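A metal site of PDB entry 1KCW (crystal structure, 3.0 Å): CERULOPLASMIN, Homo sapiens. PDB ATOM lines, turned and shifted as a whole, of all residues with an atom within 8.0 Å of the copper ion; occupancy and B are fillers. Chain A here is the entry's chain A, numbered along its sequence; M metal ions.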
ATOM      1  N   PHE A 202      27.636 -11.257  27.229  1.00  0.00           N
ATOM      2  CA  PHE A 202      26.889 -12.015  26.235  1.00  0.00           C
ATOM      3  C   PHE A 202      25.506 -12.105  26.826  1.00  0.00           C
ATOM      4  O   PHE A 202      25.385 -12.252  28.042  1.00  0.00           O
ATOM      5  CB  PHE A 202      27.463 -13.415  26.019  1.00  0.00           C
ATOM      6  CG  PHE A 202      28.644 -13.452  25.084  1.00  0.00           C
ATOM      7  CD1 PHE A 202      29.816 -12.782  25.393  1.00  0.00           C
ATOM      8  CD2 PHE A 202      28.551 -14.126  23.882  1.00  0.00           C
ATOM      9  CE1 PHE A 202      30.870 -12.786  24.533  1.00  0.00           C
ATOM     10  CE2 PHE A 202      29.615 -14.141  23.002  1.00  0.00           C
ATOM     11  CZ  PHE A 202      30.779 -13.469  23.326  1.00  0.00           C
ATOM     12  N   SER A 203      24.495 -11.937  25.971  1.00  0.00           N
ATOM     13  CA  SER A 203      23.097 -12.016  26.389  1.00  0.00           C
ATOM     14  C   SER A 203      22.110 -11.947  25.212  1.00  0.00           C
ATOM     15  O   SER A 203      22.330 -11.220  24.246  1.00  0.00           O
ATOM     16  CB  SER A 203      22.773 -10.894  27.382  1.00  0.00           C
ATOM     17  OG  SER A 203      21.376 -10.777  27.588  1.00  0.00           O
ATOM     18  N   VAL A 204      21.047 -12.743  25.314  1.00  0.00           N
ATOM     19  CA  VAL A 204      19.913 -12.668  24.394  1.00  0.00           C
ATOM     20  C   VAL A 204      18.983 -11.664  25.036  1.00  0.00           C
ATOM     21  O   VAL A 204      17.963 -12.058  25.628  1.00  0.00           O
ATOM     22  CB  VAL A 204      19.198 -14.039  24.319  1.00  0.00           C
ATOM     23  CG1 VAL A 204      18.027 -13.979  23.362  1.00  0.00           C
ATOM     24  CG2 VAL A 204      20.176 -15.137  23.942  1.00  0.00           C
ATOM     25  N   TYR A 241      19.924 -11.308  20.265  1.00  0.00           N
ATOM     26  CA  TYR A 241      21.180 -12.015  20.508  1.00  0.00           C
ATOM     27  C   TYR A 241      22.318 -11.037  20.331  1.00  0.00           C
ATOM     28  O   TYR A 241      22.624 -10.657  19.209  1.00  0.00           O
ATOM     29  CB  TYR A 241      21.270 -13.182  19.524  1.00  0.00           C
ATOM     30  CG  TYR A 241      20.130 -14.191  19.645  1.00  0.00           C
ATOM     31  CD1 TYR A 241      18.854 -13.903  19.194  1.00  0.00           C
ATOM     32  CD2 TYR A 241      20.339 -15.440  20.228  1.00  0.00           C
ATOM     33  CE1 TYR A 241      17.823 -14.850  19.317  1.00  0.00           C
ATOM     34  CE2 TYR A 241      19.313 -16.366  20.358  1.00  0.00           C
ATOM     35  CZ  TYR A 241      18.067 -16.070  19.909  1.00  0.00           C
ATOM     36  OH  TYR A 241      17.071 -17.007  20.056  1.00  0.00           O
ATOM     37  N   SER A 242      23.001 -10.654  21.402  1.00  0.00           N
ATOM     38  CA  SER A 242      24.022  -9.635  21.264  1.00  0.00           C
ATOM     39  C   SER A 242      25.024  -9.623  22.237  1.00  0.00           C
ATOM     40  O   SER A 242      24.780  -9.881  23.403  1.00  0.00           O
ATOM     41  CB  SER A 242      23.296  -8.316  21.281  1.00  0.00           C
ATOM     42  OG  SER A 242      22.490  -8.186  22.444  1.00  0.00           O
ATOM     43  N   VAL A 273      17.920 -19.919  27.923  1.00  0.00           N
ATOM     44  CA  VAL A 273      18.319 -20.183  26.553  1.00  0.00           C
ATOM     45  C   VAL A 273      19.621 -19.436  26.450  1.00  0.00           C
ATOM     46  O   VAL A 273      20.082 -19.178  25.357  1.00  0.00           O
ATOM     47  CB  VAL A 273      17.296 -19.641  25.491  1.00  0.00           C
ATOM     48  CG1 VAL A 273      15.901 -20.129  25.810  1.00  0.00           C
ATOM     49  CG2 VAL A 273      17.331 -18.127  25.413  1.00  0.00           C
ATOM     50  N   ASP A 274      20.190 -19.084  27.590  1.00  0.00           N
ATOM     51  CA  ASP A 274      21.435 -18.336  27.568  1.00  0.00           C
ATOM     52  C   ASP A 274      22.666 -19.187  27.834  1.00  0.00           C
ATOM     53  O   ASP A 274      23.439 -18.953  28.767  1.00  0.00           O
ATOM     54  CB  ASP A 274      21.364 -17.157  28.514  1.00  0.00           C
ATOM     55  CG  ASP A 274      20.741 -15.957  27.873  1.00  0.00           C
ATOM     56  OD1 ASP A 274      19.499 -15.795  27.931  1.00  0.00           O
ATOM     57  OD2 ASP A 274      21.503 -15.175  27.304  1.00  0.00           O
ATOM     58  N   VAL A 275      22.835 -20.178  26.955  1.00  0.00           N
ATOM     59  CA  VAL A 275      23.941 -21.086  27.033  1.00  0.00           C
ATOM     60  C   VAL A 275      24.915 -20.522  25.998  1.00  0.00           C
ATOM     61  O   VAL A 275      24.730 -20.708  24.801  1.00  0.00           O
ATOM     62  CB  VAL A 275      23.445 -22.460  26.641  1.00  0.00           C
ATOM     63  CG1 VAL A 275      24.578 -23.435  26.591  1.00  0.00           C
ATOM     64  CG2 VAL A 275      22.402 -22.912  27.620  1.00  0.00           C
ATOM     65  N   HIS A 276      25.891 -19.755  26.469  1.00  0.00           N
ATOM     66  CA  HIS A 276      26.847 -19.139  25.575  1.00  0.00           C
ATOM     67  C   HIS A 276      28.168 -19.848  25.505  1.00  0.00           C
ATOM     68  O   HIS A 276      28.513 -20.602  26.394  1.00  0.00           O
ATOM     69  CB  HIS A 276      27.095 -17.671  25.966  1.00  0.00           C
ATOM     70  CG  HIS A 276      25.844 -16.844  25.972  1.00  0.00           C
ATOM     71  ND1 HIS A 276      25.226 -16.499  24.809  1.00  0.00           N
ATOM     72  CD2 HIS A 276      25.038 -16.566  27.020  1.00  0.00           C
ATOM     73  CE1 HIS A 276      24.040 -16.032  25.167  1.00  0.00           C
ATOM     74  NE2 HIS A 276      23.887 -16.051  26.502  1.00  0.00           N
ATOM     75  N   ALA A 277      28.933 -19.511  24.468  1.00  0.00           N
ATOM     76  CA  ALA A 277      30.254 -20.077  24.224  1.00  0.00           C
ATOM     77  C   ALA A 277      31.073 -18.994  23.563  1.00  0.00           C
ATOM     78  O   ALA A 277      31.213 -18.979  22.347  1.00  0.00           O
ATOM     79  CB  ALA A 277      30.139 -21.267  23.314  1.00  0.00           C
ATOM     80  N   ALA A 278      31.550 -18.046  24.349  1.00  0.00           N
ATOM     81  CA  ALA A 278      32.343 -16.953  23.817  1.00  0.00           C
ATOM     82  C   ALA A 278      33.592 -17.513  23.170  1.00  0.00           C
ATOM     83  O   ALA A 278      34.275 -18.338  23.758  1.00  0.00           O
ATOM     84  CB  ALA A 278      32.723 -16.012  24.914  1.00  0.00           C
ATOM     85  N   LEU A 297      29.406 -19.051  29.243  1.00  0.00           N
ATOM     86  CA  LEU A 297      28.784 -18.053  30.090  1.00  0.00           C
ATOM     87  C   LEU A 297      27.316 -18.327  30.143  1.00  0.00           C
ATOM     88  O   LEU A 297      26.700 -18.624  29.123  1.00  0.00           O
ATOM     89  CB  LEU A 297      28.984 -16.680  29.480  1.00  0.00           C
ATOM     90  CG  LEU A 297      30.459 -16.274  29.396  1.00  0.00           C
ATOM     91  CD1 LEU A 297      30.621 -14.898  28.734  1.00  0.00           C
ATOM     92  CD2 LEU A 297      31.059 -16.264  30.782  1.00  0.00           C
ATOM     93  N   SER A 318      32.654 -14.575  18.664  1.00  0.00           N
ATOM     94  CA  SER A 318      31.304 -15.060  18.463  1.00  0.00           C
ATOM     95  C   SER A 318      30.904 -15.977  19.601  1.00  0.00           C
ATOM     96  O   SER A 318      31.688 -16.196  20.528  1.00  0.00           O
ATOM     97  CB  SER A 318      31.153 -15.768  17.111  1.00  0.00           C
ATOM     98  OG  SER A 318      31.948 -16.930  17.046  1.00  0.00           O
ATOM     99  N   CYS A 319      29.685 -16.475  19.548  1.00  0.00           N
ATOM    100  CA  CYS A 319      29.225 -17.374  20.568  1.00  0.00           C
ATOM    101  C   CYS A 319      28.970 -18.704  19.844  1.00  0.00           C
ATOM    102  O   CYS A 319      27.975 -18.851  19.126  1.00  0.00           O
ATOM    103  CB  CYS A 319      27.960 -16.811  21.200  1.00  0.00           C
ATOM    104  SG  CYS A 319      27.051 -17.951  22.161  1.00  0.00           S
ATOM    105  N   GLN A 320      29.885 -19.653  20.018  1.00  0.00           N
ATOM    106  CA  GLN A 320      29.797 -20.945  19.356  1.00  0.00           C
ATOM    107  C   GLN A 320      28.522 -21.718  19.575  1.00  0.00           C
ATOM    108  O   GLN A 320      28.343 -22.805  19.004  1.00  0.00           O
ATOM    109  CB  GLN A 320      31.007 -21.795  19.677  1.00  0.00           C
ATOM    110  CG  GLN A 320      32.291 -21.297  19.064  1.00  0.00           C
ATOM    111  CD  GLN A 320      32.051 -20.770  17.669  1.00  0.00           C
ATOM    112  OE1 GLN A 320      31.464 -21.464  16.841  1.00  0.00           O
ATOM    113  NE2 GLN A 320      32.432 -19.594  17.209  1.00  0.00           N
ATOM    114  N   ASN A 321      27.627 -21.242  20.402  1.00  0.00           N
ATOM    115  CA  ASN A 321      26.337 -21.888  20.447  1.00  0.00           C
ATOM    116  C   ASN A 321      25.791 -21.714  19.041  1.00  0.00           C
ATOM    117  O   ASN A 321      25.650 -20.587  18.578  1.00  0.00           O
ATOM    118  CB  ASN A 321      25.459 -21.249  21.512  1.00  0.00           C
ATOM    119  CG  ASN A 321      24.031 -21.730  21.447  1.00  0.00           C
ATOM    120  OD1 ASN A 321      23.563 -22.185  20.410  1.00  0.00           O
ATOM    121  ND2 ASN A 321      23.339 -21.632  22.574  1.00  0.00           N
ATOM    122  N   LEU A 322      25.514 -22.808  18.336  1.00  0.00           N
ATOM    123  CA  LEU A 322      25.032 -22.690  16.963  1.00  0.00           C
ATOM    124  C   LEU A 322      23.832 -21.811  16.775  1.00  0.00           C
ATOM    125  O   LEU A 322      23.903 -20.862  15.999  1.00  0.00           O
ATOM    126  CB  LEU A 322      24.767 -24.052  16.323  1.00  0.00           C
ATOM    127  CG  LEU A 322      25.997 -24.965  16.269  1.00  0.00           C
ATOM    128  CD1 LEU A 322      25.541 -26.282  15.688  1.00  0.00           C
ATOM    129  CD2 LEU A 322      27.190 -24.374  15.487  1.00  0.00           C
ATOM    130  N   ASN A 323      22.752 -22.073  17.510  1.00  0.00           N
ATOM    131  CA  ASN A 323      21.566 -21.232  17.359  1.00  0.00           C
ATOM    132  C   ASN A 323      21.814 -19.741  17.564  1.00  0.00           C
ATOM    133  O   ASN A 323      21.232 -18.905  16.870  1.00  0.00           O
ATOM    134  CB  ASN A 323      20.453 -21.736  18.243  1.00  0.00           C
ATOM    135  CG  ASN A 323      19.806 -22.951  17.676  1.00  0.00           C
ATOM    136  OD1 ASN A 323      20.317 -23.547  16.717  1.00  0.00           O
ATOM    137  ND2 ASN A 323      18.659 -23.333  18.221  1.00  0.00           N
ATOM    138  N   HIS A 324      22.713 -19.400  18.463  1.00  0.00           N
ATOM    139  CA  HIS A 324      23.017 -18.021  18.717  1.00  0.00           C
ATOM    140  C   HIS A 324      23.832 -17.497  17.559  1.00  0.00           C
ATOM    141  O   HIS A 324      23.587 -16.406  17.067  1.00  0.00           O
ATOM    142  CB  HIS A 324      23.742 -17.869  20.072  1.00  0.00           C
ATOM    143  CG  HIS A 324      22.876 -18.191  21.258  1.00  0.00           C
ATOM    144  ND1 HIS A 324      23.338 -18.121  22.540  1.00  0.00           N
ATOM    145  CD2 HIS A 324      21.618 -18.719  21.267  1.00  0.00           C
ATOM    146  CE1 HIS A 324      22.396 -18.602  23.307  1.00  0.00           C
ATOM    147  NE2 HIS A 324      21.326 -18.991  22.573  1.00  0.00           N
ATOM    148  N   LEU A 325      24.733 -18.319  17.044  1.00  0.00           N
ATOM    149  CA  LEU A 325      25.567 -17.908  15.916  1.00  0.00           C
ATOM    150  C   LEU A 325      24.729 -17.497  14.683  1.00  0.00           C
ATOM    151  O   LEU A 325      25.021 -16.488  14.047  1.00  0.00           O
ATOM    152  CB  LEU A 325      26.504 -19.041  15.542  1.00  0.00           C
ATOM    153  CG  LEU A 325      27.498 -18.720  14.429  1.00  0.00           C
ATOM    154  CD1 LEU A 325      28.774 -18.122  15.035  1.00  0.00           C
ATOM    155  CD2 LEU A 325      27.840 -20.006  13.687  1.00  0.00           C
ATOM    156  N   LEU A 329      25.099 -13.410  16.581  1.00  0.00           N
ATOM    157  CA  LEU A 329      25.759 -12.964  17.789  1.00  0.00           C
ATOM    158  C   LEU A 329      27.225 -12.920  17.455  1.00  0.00           C
ATOM    159  O   LEU A 329      28.017 -13.683  18.001  1.00  0.00           O
ATOM    160  CB  LEU A 329      25.521 -13.941  18.953  1.00  0.00           C
ATOM    161  CG  LEU A 329      25.640 -13.332  20.372  1.00  0.00           C
ATOM    162  CD1 LEU A 329      24.888 -14.193  21.341  1.00  0.00           C
ATOM    163  CD2 LEU A 329      27.073 -13.120  20.824  1.00  0.00           C
ATOM    164  N   GLU A 633      21.851 -24.864  22.526  1.00  0.00           N
ATOM    165  CA  GLU A 633      21.632 -24.682  23.953  1.00  0.00           C
ATOM    166  C   GLU A 633      21.074 -25.912  24.635  1.00  0.00           C
ATOM    167  O   GLU A 633      20.775 -25.894  25.837  1.00  0.00           O
ATOM    168  CB  GLU A 633      20.735 -23.471  24.214  1.00  0.00           C
ATOM    169  CG  GLU A 633      19.272 -23.647  23.788  1.00  0.00           C
ATOM    170  CD  GLU A 633      18.975 -23.076  22.410  1.00  0.00           C
ATOM    171  OE1 GLU A 633      19.782 -22.280  21.862  1.00  0.00           O
ATOM    172  OE2 GLU A 633      17.897 -23.427  21.876  1.00  0.00           O
ATOM    173  N   PRO A 660      28.187 -26.282  24.546  1.00  0.00           N
ATOM    174  CA  PRO A 660      28.707 -25.992  23.212  1.00  0.00           C
ATOM    175  C   PRO A 660      30.186 -25.609  23.152  1.00  0.00           C
ATOM    176  O   PRO A 660      30.571 -24.556  23.649  1.00  0.00           O
ATOM    177  CB  PRO A 660      27.824 -24.846  22.770  1.00  0.00           C
ATOM    178  CG  PRO A 660      26.488 -25.274  23.327  1.00  0.00           C
ATOM    179  CD  PRO A 660      26.871 -25.652  24.733  1.00  0.00           C
HETATM  180 CU    CU M   1      25.251 -17.517  22.971  1.00  0.00          CU
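N of Asn 321 sits close to SG of Cys 319 (3.8 Å). The side-chain sulfur (SG) of Cys 319 lies close to the backbone NH (N) of Ala 277, at 3.4 Å. N of Leu 329 is in hydrogen-bond range of O of His 324, at 3.4 Å. A ring nitrogen (NE2) of His 324 sits close to the side-chain amide nitrogen (ND2) of Asn 321 (3.3 Å). A ring nitrogen (NE2) of His 324 lies within hydrogen-bond range of the backbone carbonyl oxygen of Val 273 (3.1 Å). OD2 of Asp 274 lies within hydrogen-bond range of NE2 of His 276, at 2.7 Å. O of Leu 297 is in hydrogen-bond range of N of His 276 (3.0 Å). The backbone carbonyl oxygen (O) of Val 275 sits at hydrogen-bond distance from the side-chain amide nitrogen (ND2) of Asn 321 (2.8 Å).
Val 275 touches the copper ion. CD1 of Leu 329 touches the copper ion, 3.7 Å away. The nearest printed residue that does not touch the copper ion is Asn 321 (4.01 Å).
The copper ion is bound by SG of Cys 319 (2.0 Å). The copper ion is bound by ND1 of His 324 (2.1 Å). The copper ion is bound by a ring nitrogen (ND1) of His 276, 2.1 Å away. The copper ion has three donor atoms within binding distance.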
